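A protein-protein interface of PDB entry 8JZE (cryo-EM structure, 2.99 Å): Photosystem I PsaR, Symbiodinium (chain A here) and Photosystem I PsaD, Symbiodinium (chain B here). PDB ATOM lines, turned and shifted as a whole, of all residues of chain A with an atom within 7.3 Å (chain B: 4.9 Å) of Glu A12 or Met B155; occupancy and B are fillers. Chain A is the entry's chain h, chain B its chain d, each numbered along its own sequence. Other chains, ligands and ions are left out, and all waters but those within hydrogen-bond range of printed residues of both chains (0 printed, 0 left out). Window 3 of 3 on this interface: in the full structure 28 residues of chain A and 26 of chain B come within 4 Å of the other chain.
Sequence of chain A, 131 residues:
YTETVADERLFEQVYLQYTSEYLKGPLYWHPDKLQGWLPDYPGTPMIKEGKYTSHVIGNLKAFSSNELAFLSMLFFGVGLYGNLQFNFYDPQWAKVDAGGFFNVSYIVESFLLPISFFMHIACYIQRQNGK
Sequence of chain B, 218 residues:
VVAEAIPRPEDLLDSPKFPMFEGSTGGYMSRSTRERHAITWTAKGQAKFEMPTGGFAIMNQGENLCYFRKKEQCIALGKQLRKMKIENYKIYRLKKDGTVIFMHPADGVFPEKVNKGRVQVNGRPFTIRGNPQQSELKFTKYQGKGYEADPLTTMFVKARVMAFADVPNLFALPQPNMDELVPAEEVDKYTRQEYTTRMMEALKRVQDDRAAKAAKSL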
ATOM      1  N   VAL A   5       2.750 -15.656   0.101  1.00  0.00           N
ATOM      2  CA  VAL A   5       1.491 -15.916  -0.593  1.00  0.00           C
ATOM      3  C   VAL A   5       1.043 -17.355  -0.375  1.00  0.00           C
ATOM      4  O   VAL A   5      -0.160 -17.644  -0.361  1.00  0.00           O
ATOM      5  CB  VAL A   5       1.632 -15.578  -2.089  1.00  0.00           C
ATOM      6  CG1 VAL A   5       2.115 -14.148  -2.250  1.00  0.00           C
ATOM      7  CG2 VAL A   5       2.584 -16.546  -2.770  1.00  0.00           C
ATOM      8  N   ALA A   6       1.994 -18.275  -0.198  1.00  0.00           N
ATOM      9  CA  ALA A   6       1.643 -19.655   0.112  1.00  0.00           C
ATOM     10  C   ALA A   6       0.962 -19.756   1.470  1.00  0.00           C
ATOM     11  O   ALA A   6       0.022 -20.536   1.640  1.00  0.00           O
ATOM     12  CB  ALA A   6       2.888 -20.540   0.068  1.00  0.00           C
ATOM     13  N   ASP A   7       1.428 -18.981   2.451  1.00  0.00           N
ATOM     14  CA  ASP A   7       0.790 -18.986   3.765  1.00  0.00           C
ATOM     15  C   ASP A   7      -0.616 -18.403   3.698  1.00  0.00           C
ATOM     16  O   ASP A   7      -1.536 -18.906   4.357  1.00  0.00           O
ATOM     17  CB  ASP A   7       1.649 -18.213   4.765  1.00  0.00           C
ATOM     18  CG  ASP A   7       3.071 -18.736   4.836  1.00  0.00           C
ATOM     19  OD1 ASP A   7       3.264 -19.960   4.679  1.00  0.00           O
ATOM     20  OD2 ASP A   7       3.995 -17.921   5.042  1.00  0.00           O
ATOM     21  N   GLU A   8      -0.805 -17.342   2.910  1.00  0.00           N
ATOM     22  CA  GLU A   8      -2.146 -16.800   2.720  1.00  0.00           C
ATOM     23  C   GLU A   8      -3.058 -17.825   2.059  1.00  0.00           C
ATOM     24  O   GLU A   8      -4.214 -17.984   2.458  1.00  0.00           O
ATOM     25  CB  GLU A   8      -2.092 -15.518   1.889  1.00  0.00           C
ATOM     26  CG  GLU A   8      -1.375 -14.357   2.559  1.00  0.00           C
ATOM     27  CD  GLU A   8      -1.544 -13.053   1.802  1.00  0.00           C
ATOM     28  OE1 GLU A   8      -2.205 -13.060   0.742  1.00  0.00           O
ATOM     29  OE2 GLU A   8      -1.021 -12.019   2.268  1.00  0.00           O
ATOM     30  N   ARG A   9      -2.549 -18.535   1.048  1.00  0.00           N
ATOM     31  CA  ARG A   9      -3.333 -19.584   0.401  1.00  0.00           C
ATOM     32  C   ARG A   9      -3.667 -20.705   1.379  1.00  0.00           C
ATOM     33  O   ARG A   9      -4.768 -21.269   1.342  1.00  0.00           O
ATOM     34  CB  ARG A   9      -2.568 -20.121  -0.811  1.00  0.00           C
ATOM     35  CG  ARG A   9      -3.168 -21.352  -1.463  1.00  0.00           C
ATOM     36  CD  ARG A   9      -4.587 -21.108  -1.937  1.00  0.00           C
ATOM     37  NE  ARG A   9      -5.117 -22.264  -2.647  1.00  0.00           N
ATOM     38  CZ  ARG A   9      -5.252 -22.336  -3.963  1.00  0.00           C
ATOM     39  NH1 ARG A   9      -4.942 -21.315  -4.743  1.00  0.00           N
ATOM     40  NH2 ARG A   9      -5.716 -23.456  -4.509  1.00  0.00           N
ATOM     41  N   LEU A  10      -2.723 -21.046   2.258  1.00  0.00           N
ATOM     42  CA  LEU A  10      -2.986 -22.048   3.285  1.00  0.00           C
ATOM     43  C   LEU A  10      -4.095 -21.594   4.223  1.00  0.00           C
ATOM     44  O   LEU A  10      -4.958 -22.392   4.606  1.00  0.00           O
ATOM     45  CB  LEU A  10      -1.707 -22.340   4.069  1.00  0.00           C
ATOM     46  CG  LEU A  10      -1.867 -23.174   5.341  1.00  0.00           C
ATOM     47  CD1 LEU A  10      -2.276 -24.596   5.001  1.00  0.00           C
ATOM     48  CD2 LEU A  10      -0.590 -23.161   6.165  1.00  0.00           C
ATOM     49  N   PHE A  11      -4.082 -20.318   4.614  1.00  0.00           N
ATOM     50  CA  PHE A  11      -5.169 -19.808   5.444  1.00  0.00           C
ATOM     51  C   PHE A  11      -6.490 -19.847   4.691  1.00  0.00           C
ATOM     52  O   PHE A  11      -7.535 -20.141   5.278  1.00  0.00           O
ATOM     53  CB  PHE A  11      -4.879 -18.388   5.925  1.00  0.00           C
ATOM     54  CG  PHE A  11      -5.938 -17.840   6.846  1.00  0.00           C
ATOM     55  CD1 PHE A  11      -5.879 -18.083   8.209  1.00  0.00           C
ATOM     56  CD2 PHE A  11      -6.998 -17.098   6.349  1.00  0.00           C
ATOM     57  CE1 PHE A  11      -6.851 -17.590   9.060  1.00  0.00           C
ATOM     58  CE2 PHE A  11      -7.975 -16.601   7.194  1.00  0.00           C
ATOM     59  CZ  PHE A  11      -7.900 -16.849   8.552  1.00  0.00           C
ATOM     60  N   GLU A  12      -6.465 -19.534   3.394  1.00  0.00           N
ATOM     61  CA  GLU A  12      -7.673 -19.649   2.580  1.00  0.00           C
ATOM     62  C   GLU A  12      -8.223 -21.067   2.638  1.00  0.00           C
ATOM     63  O   GLU A  12      -9.419 -21.276   2.861  1.00  0.00           O
ATOM     64  CB  GLU A  12      -7.381 -19.261   1.128  1.00  0.00           C
ATOM     65  CG  GLU A  12      -6.781 -17.882   0.924  1.00  0.00           C
ATOM     66  CD  GLU A  12      -7.821 -16.798   0.781  1.00  0.00           C
ATOM     67  OE1 GLU A  12      -8.914 -17.088   0.254  1.00  0.00           O
ATOM     68  OE2 GLU A  12      -7.543 -15.653   1.196  1.00  0.00           O
ATOM     69  N   GLN A  13      -7.349 -22.058   2.439  1.00  0.00           N
ATOM     70  CA  GLN A  13      -7.788 -23.450   2.436  1.00  0.00           C
ATOM     71  C   GLN A  13      -8.332 -23.864   3.796  1.00  0.00           C
ATOM     72  O   GLN A  13      -9.377 -24.518   3.880  1.00  0.00           O
ATOM     73  CB  GLN A  13      -6.635 -24.362   2.016  1.00  0.00           C
ATOM     74  CG  GLN A  13      -6.117 -24.095   0.614  1.00  0.00           C
ATOM     75  CD  GLN A  13      -7.172 -24.329  -0.449  1.00  0.00           C
ATOM     76  OE1 GLN A  13      -7.539 -23.415  -1.188  1.00  0.00           O
ATOM     77  NE2 GLN A  13      -7.662 -25.559  -0.534  1.00  0.00           N
ATOM     78  N   VAL A  14      -7.641 -23.484   4.875  1.00  0.00           N
ATOM     79  CA  VAL A  14      -8.095 -23.840   6.219  1.00  0.00           C
ATOM     80  C   VAL A  14      -9.449 -23.205   6.507  1.00  0.00           C
ATOM     81  O   VAL A  14     -10.376 -23.867   6.996  1.00  0.00           O
ATOM     82  CB  VAL A  14      -7.044 -23.425   7.265  1.00  0.00           C
ATOM     83  CG1 VAL A  14      -7.636 -23.483   8.662  1.00  0.00           C
ATOM     84  CG2 VAL A  14      -5.825 -24.320   7.171  1.00  0.00           C
ATOM     85  N   TYR A  15      -9.584 -21.913   6.201  1.00  0.00           N
ATOM     86  CA  TYR A  15     -10.831 -21.202   6.454  1.00  0.00           C
ATOM     87  C   TYR A  15     -11.978 -21.817   5.668  1.00  0.00           C
ATOM     88  O   TYR A  15     -13.067 -22.031   6.208  1.00  0.00           O
ATOM     89  CB  TYR A  15     -10.665 -19.722   6.099  1.00  0.00           C
ATOM     90  CG  TYR A  15     -11.906 -18.877   6.298  1.00  0.00           C
ATOM     91  CD1 TYR A  15     -12.885 -18.794   5.313  1.00  0.00           C
ATOM     92  CD2 TYR A  15     -12.089 -18.146   7.462  1.00  0.00           C
ATOM     93  CE1 TYR A  15     -14.013 -18.023   5.491  1.00  0.00           C
ATOM     94  CE2 TYR A  15     -13.212 -17.368   7.647  1.00  0.00           C
ATOM     95  CZ  TYR A  15     -14.173 -17.313   6.659  1.00  0.00           C
ATOM     96  OH  TYR A  15     -15.297 -16.541   6.837  1.00  0.00           O
ATOM     97  N   LEU A  16     -11.755 -22.103   4.383  1.00  0.00           N
ATOM     98  CA  LEU A  16     -12.821 -22.672   3.566  1.00  0.00           C
ATOM     99  C   LEU A  16     -13.200 -24.067   4.044  1.00  0.00           C
ATOM    100  O   LEU A  16     -14.388 -24.386   4.152  1.00  0.00           O
ATOM    101  CB  LEU A  16     -12.403 -22.695   2.096  1.00  0.00           C
ATOM    102  CG  LEU A  16     -12.280 -21.329   1.417  1.00  0.00           C
ATOM    103  CD1 LEU A  16     -11.840 -21.477  -0.027  1.00  0.00           C
ATOM    104  CD2 LEU A  16     -13.590 -20.574   1.500  1.00  0.00           C
ATOM    105  N   GLN A  17     -12.208 -24.906   4.355  1.00  0.00           N
ATOM    106  CA  GLN A  17     -12.501 -26.262   4.803  1.00  0.00           C
ATOM    107  C   GLN A  17     -13.269 -26.254   6.117  1.00  0.00           C
ATOM    108  O   GLN A  17     -14.185 -27.062   6.312  1.00  0.00           O
ATOM    109  CB  GLN A  17     -11.201 -27.060   4.930  1.00  0.00           C
ATOM    110  CG  GLN A  17     -11.387 -28.545   5.215  1.00  0.00           C
ATOM    111  CD  GLN A  17     -11.541 -28.848   6.692  1.00  0.00           C
ATOM    112  OE1 GLN A  17     -11.120 -28.067   7.546  1.00  0.00           O
ATOM    113  NE2 GLN A  17     -12.151 -29.985   7.003  1.00  0.00           N
ATOM    114  N   TYR A  18     -12.914 -25.352   7.035  1.00  0.00           N
ATOM    115  CA  TYR A  18     -13.638 -25.281   8.301  1.00  0.00           C
ATOM    116  C   TYR A  18     -15.042 -24.719   8.108  1.00  0.00           C
ATOM    117  O   TYR A  18     -16.021 -25.270   8.627  1.00  0.00           O
ATOM    118  CB  TYR A  18     -12.861 -24.438   9.311  1.00  0.00           C
ATOM    119  CG  TYR A  18     -13.651 -24.139  10.562  1.00  0.00           C
ATOM    120  CD1 TYR A  18     -13.777 -25.087  11.569  1.00  0.00           C
ATOM    121  CD2 TYR A  18     -14.280 -22.913  10.735  1.00  0.00           C
ATOM    122  CE1 TYR A  18     -14.503 -24.822  12.712  1.00  0.00           C
ATOM    123  CE2 TYR A  18     -15.008 -22.639  11.874  1.00  0.00           C
ATOM    124  CZ  TYR A  18     -15.116 -23.597  12.858  1.00  0.00           C
ATOM    125  OH  TYR A  18     -15.841 -23.325  13.993  1.00  0.00           O
ATOM    126  N   THR A  19     -15.162 -23.619   7.361  1.00  0.00           N
ATOM    127  CA  THR A  19     -16.442 -22.930   7.264  1.00  0.00           C
ATOM    128  C   THR A  19     -17.446 -23.725   6.442  1.00  0.00           C
ATOM    129  O   THR A  19     -18.638 -23.728   6.755  1.00  0.00           O
ATOM    130  CB  THR A  19     -16.243 -21.534   6.677  1.00  0.00           C
ATOM    131  OG1 THR A  19     -15.250 -20.835   7.438  1.00  0.00           O
ATOM    132  CG2 THR A  19     -17.538 -20.747   6.729  1.00  0.00           C
ATOM    133  N   LEU A  23     -21.067 -24.418   8.096  1.00  0.00           N
ATOM    134  CA  LEU A  23     -22.316 -23.862   7.584  1.00  0.00           C
ATOM    135  C   LEU A  23     -23.363 -24.942   7.346  1.00  0.00           C
ATOM    136  O   LEU A  23     -24.563 -24.651   7.363  1.00  0.00           O
ATOM    137  CB  LEU A  23     -22.060 -23.076   6.296  1.00  0.00           C
ATOM    138  CG  LEU A  23     -21.063 -21.918   6.393  1.00  0.00           C
ATOM    139  CD1 LEU A  23     -21.035 -21.096   5.119  1.00  0.00           C
ATOM    140  CD2 LEU A  23     -21.354 -21.037   7.591  1.00  0.00           C
ATOM    141  N   PRO B 151     -12.595  -9.084   0.728  1.00  0.00           N
ATOM    142  CA  PRO B 151     -12.159 -10.476   0.526  1.00  0.00           C
ATOM    143  C   PRO B 151     -12.717 -11.446   1.554  1.00  0.00           C
ATOM    144  O   PRO B 151     -12.921 -12.622   1.229  1.00  0.00           O
ATOM    145  CB  PRO B 151     -10.629 -10.384   0.601  1.00  0.00           C
ATOM    146  CG  PRO B 151     -10.342  -9.086   1.274  1.00  0.00           C
ATOM    147  CD  PRO B 151     -11.453  -8.168   0.881  1.00  0.00           C
ATOM    148  N   LEU B 152     -12.975 -10.991   2.783  1.00  0.00           N
ATOM    149  CA  LEU B 152     -13.586 -11.870   3.773  1.00  0.00           C
ATOM    150  C   LEU B 152     -14.979 -12.304   3.338  1.00  0.00           C
ATOM    151  O   LEU B 152     -15.344 -13.475   3.486  1.00  0.00           O
ATOM    152  CB  LEU B 152     -13.639 -11.185   5.138  1.00  0.00           C
ATOM    153  CG  LEU B 152     -14.265 -12.033   6.249  1.00  0.00           C
ATOM    154  CD1 LEU B 152     -13.540 -13.359   6.368  1.00  0.00           C
ATOM    155  CD2 LEU B 152     -14.259 -11.297   7.579  1.00  0.00           C
ATOM    156  N   THR B 153     -15.774 -11.376   2.800  1.00  0.00           N
ATOM    157  CA  THR B 153     -17.097 -11.744   2.304  1.00  0.00           C
ATOM    158  C   THR B 153     -16.996 -12.701   1.124  1.00  0.00           C
ATOM    159  O   THR B 153     -17.816 -13.619   0.989  1.00  0.00           O
ATOM    160  CB  THR B 153     -17.886 -10.495   1.912  1.00  0.00           C
ATOM    161  OG1 THR B 153     -17.044  -9.610   1.164  1.00  0.00           O
ATOM    162  CG2 THR B 153     -18.406  -9.780   3.148  1.00  0.00           C
ATOM    163  N   THR B 154     -16.003 -12.499   0.253  1.00  0.00           N
ATOM    164  CA  THR B 154     -15.817 -13.410  -0.871  1.00  0.00           C
ATOM    165  C   THR B 154     -15.491 -14.817  -0.387  1.00  0.00           C
ATOM    166  O   THR B 154     -16.051 -15.799  -0.886  1.00  0.00           O
ATOM    167  CB  THR B 154     -14.711 -12.900  -1.791  1.00  0.00           C
ATOM    168  OG1 THR B 154     -13.436 -13.174  -1.201  1.00  0.00           O
ATOM    169  CG2 THR B 154     -14.844 -11.407  -2.001  1.00  0.00           C
ATOM    170  N   MET B 155     -14.598 -14.933   0.598  1.00  0.00           N
ATOM    171  CA  MET B 155     -14.289 -16.248   1.153  1.00  0.00           C
ATOM    172  C   MET B 155     -15.503 -16.856   1.844  1.00  0.00           C
ATOM    173  O   MET B 155     -15.728 -18.068   1.763  1.00  0.00           O
ATOM    174  CB  MET B 155     -13.122 -16.156   2.131  1.00  0.00           C
ATOM    175  CG  MET B 155     -11.762 -15.992   1.491  1.00  0.00           C
ATOM    176  SD  MET B 155     -10.482 -16.041   2.755  1.00  0.00           S
ATOM    177  CE  MET B 155     -11.247 -15.036   4.019  1.00  0.00           C
ATOM    178  N   PHE B 156     -16.286 -16.035   2.546  1.00  0.00           N
ATOM    179  CA  PHE B 156     -17.459 -16.549   3.245  1.00  0.00           C
ATOM    180  C   PHE B 156     -18.481 -17.108   2.263  1.00  0.00           C
ATOM    181  O   PHE B 156     -19.021 -18.203   2.462  1.00  0.00           O
ATOM    182  CB  PHE B 156     -18.077 -15.445   4.101  1.00  0.00           C
ATOM    183  CG  PHE B 156     -19.028 -15.946   5.147  1.00  0.00           C
ATOM    184  CD1 PHE B 156     -18.558 -16.369   6.378  1.00  0.00           C
ATOM    185  CD2 PHE B 156     -20.391 -15.982   4.905  1.00  0.00           C
ATOM    186  CE1 PHE B 156     -19.427 -16.827   7.347  1.00  0.00           C
ATOM    187  CE2 PHE B 156     -21.266 -16.439   5.870  1.00  0.00           C
ATOM    188  CZ  PHE B 156     -20.783 -16.862   7.093  1.00  0.00           C
ATOM    189  N   VAL B 157     -18.749 -16.375   1.180  1.00  0.00           N
ATOM    190  CA  VAL B 157     -19.709 -16.866   0.198  1.00  0.00           C
ATOM    191  C   VAL B 157     -19.140 -18.055  -0.569  1.00  0.00           C
ATOM    192  O   VAL B 157     -19.890 -18.941  -0.988  1.00  0.00           O
ATOM    193  CB  VAL B 157     -20.160 -15.735  -0.746  1.00  0.00           C
ATOM    194  CG1 VAL B 157     -20.780 -14.598   0.045  1.00  0.00           C
ATOM    195  CG2 VAL B 157     -19.012 -15.236  -1.586  1.00  0.00           C
ATOM    196  N   LYS B 158     -17.818 -18.108  -0.761  1.00  0.00           N
ATOM    197  CA  LYS B 158     -17.210 -19.279  -1.386  1.00  0.00           C
ATOM    198  C   LYS B 158     -17.384 -20.517  -0.514  1.00  0.00           C
ATOM    199  O   LYS B 158     -17.707 -21.602  -1.013  1.00  0.00           O
ATOM    200  CB  LYS B 158     -15.731 -19.010  -1.655  1.00  0.00           C
ATOM    201  CG  LYS B 158     -15.037 -20.039  -2.529  1.00  0.00           C
ATOM    202  CD  LYS B 158     -13.624 -19.585  -2.864  1.00  0.00           C
ATOM    203  CE  LYS B 158     -12.917 -20.581  -3.764  1.00  0.00           C
ATOM    204  NZ  LYS B 158     -11.548 -20.121  -4.132  1.00  0.00           N
ATOM    205  N   ALA B 159     -17.179 -20.369   0.795  1.00  0.00           N
ATOM    206  CA  ALA B 159     -17.403 -21.479   1.713  1.00  0.00           C
ATOM    207  C   ALA B 159     -18.870 -21.880   1.735  1.00  0.00           C
ATOM    208  O   ALA B 159     -19.196 -23.068   1.839  1.00  0.00           O
ATOM    209  CB  ALA B 159     -16.921 -21.106   3.114  1.00  0.00           C
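The backbone carbonyl oxygen (O) of Tyr A15 is in hydrogen-bond range of the side-chain hydroxyl (OG1) of Thr A19 (2.8 Å).
The side-chain carboxylate of Glu A12 sits close to the side-chain sulfur of Met B155, 3.1 Å away.
Printed residues of chain A that touch a printed residue of chain B: Glu A12, Tyr A15, Leu A16 and Thr A19.
Hydrophobic or aromatic side chains of chain A that line the printed part of chain B: Tyr A15 and Leu A16.
OH of Tyr A15 touches CD1 of Leu B152 (3.7 Å).
CE1 of Tyr A15 touches CB of Met B155, at 3.9 Å.
Phe B156 touches Tyr A15 (CD1 to OH, 3.3 Å).
Leu A16 touches Met B155.
Leu A16 touches Lys B158 (CD1 to CD, 3.8 Å).
Leu A16 touches Ala B159 (CD2 to N, 3.7 Å).
Thr A19 touches Ala B159.
Glu A8 touches none of the printed residues of chain B.
Of chain B, only Met B155 comes within 4 Å of Glu A12.
Of the printed residues of chain B, Leu A16 touches Met B155, Lys B158 and Ala B159.
Of the printed residues of chain A, Leu B152 touches Tyr A15.
Met B155 touches three residues of chain A.
The nearest residue of chain A that does not touch Met B155 is Phe A11 (4.8 Å).
The nearest printed residue of chain A that does not touch Phe B156 is Leu A23 (4.2 Å).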
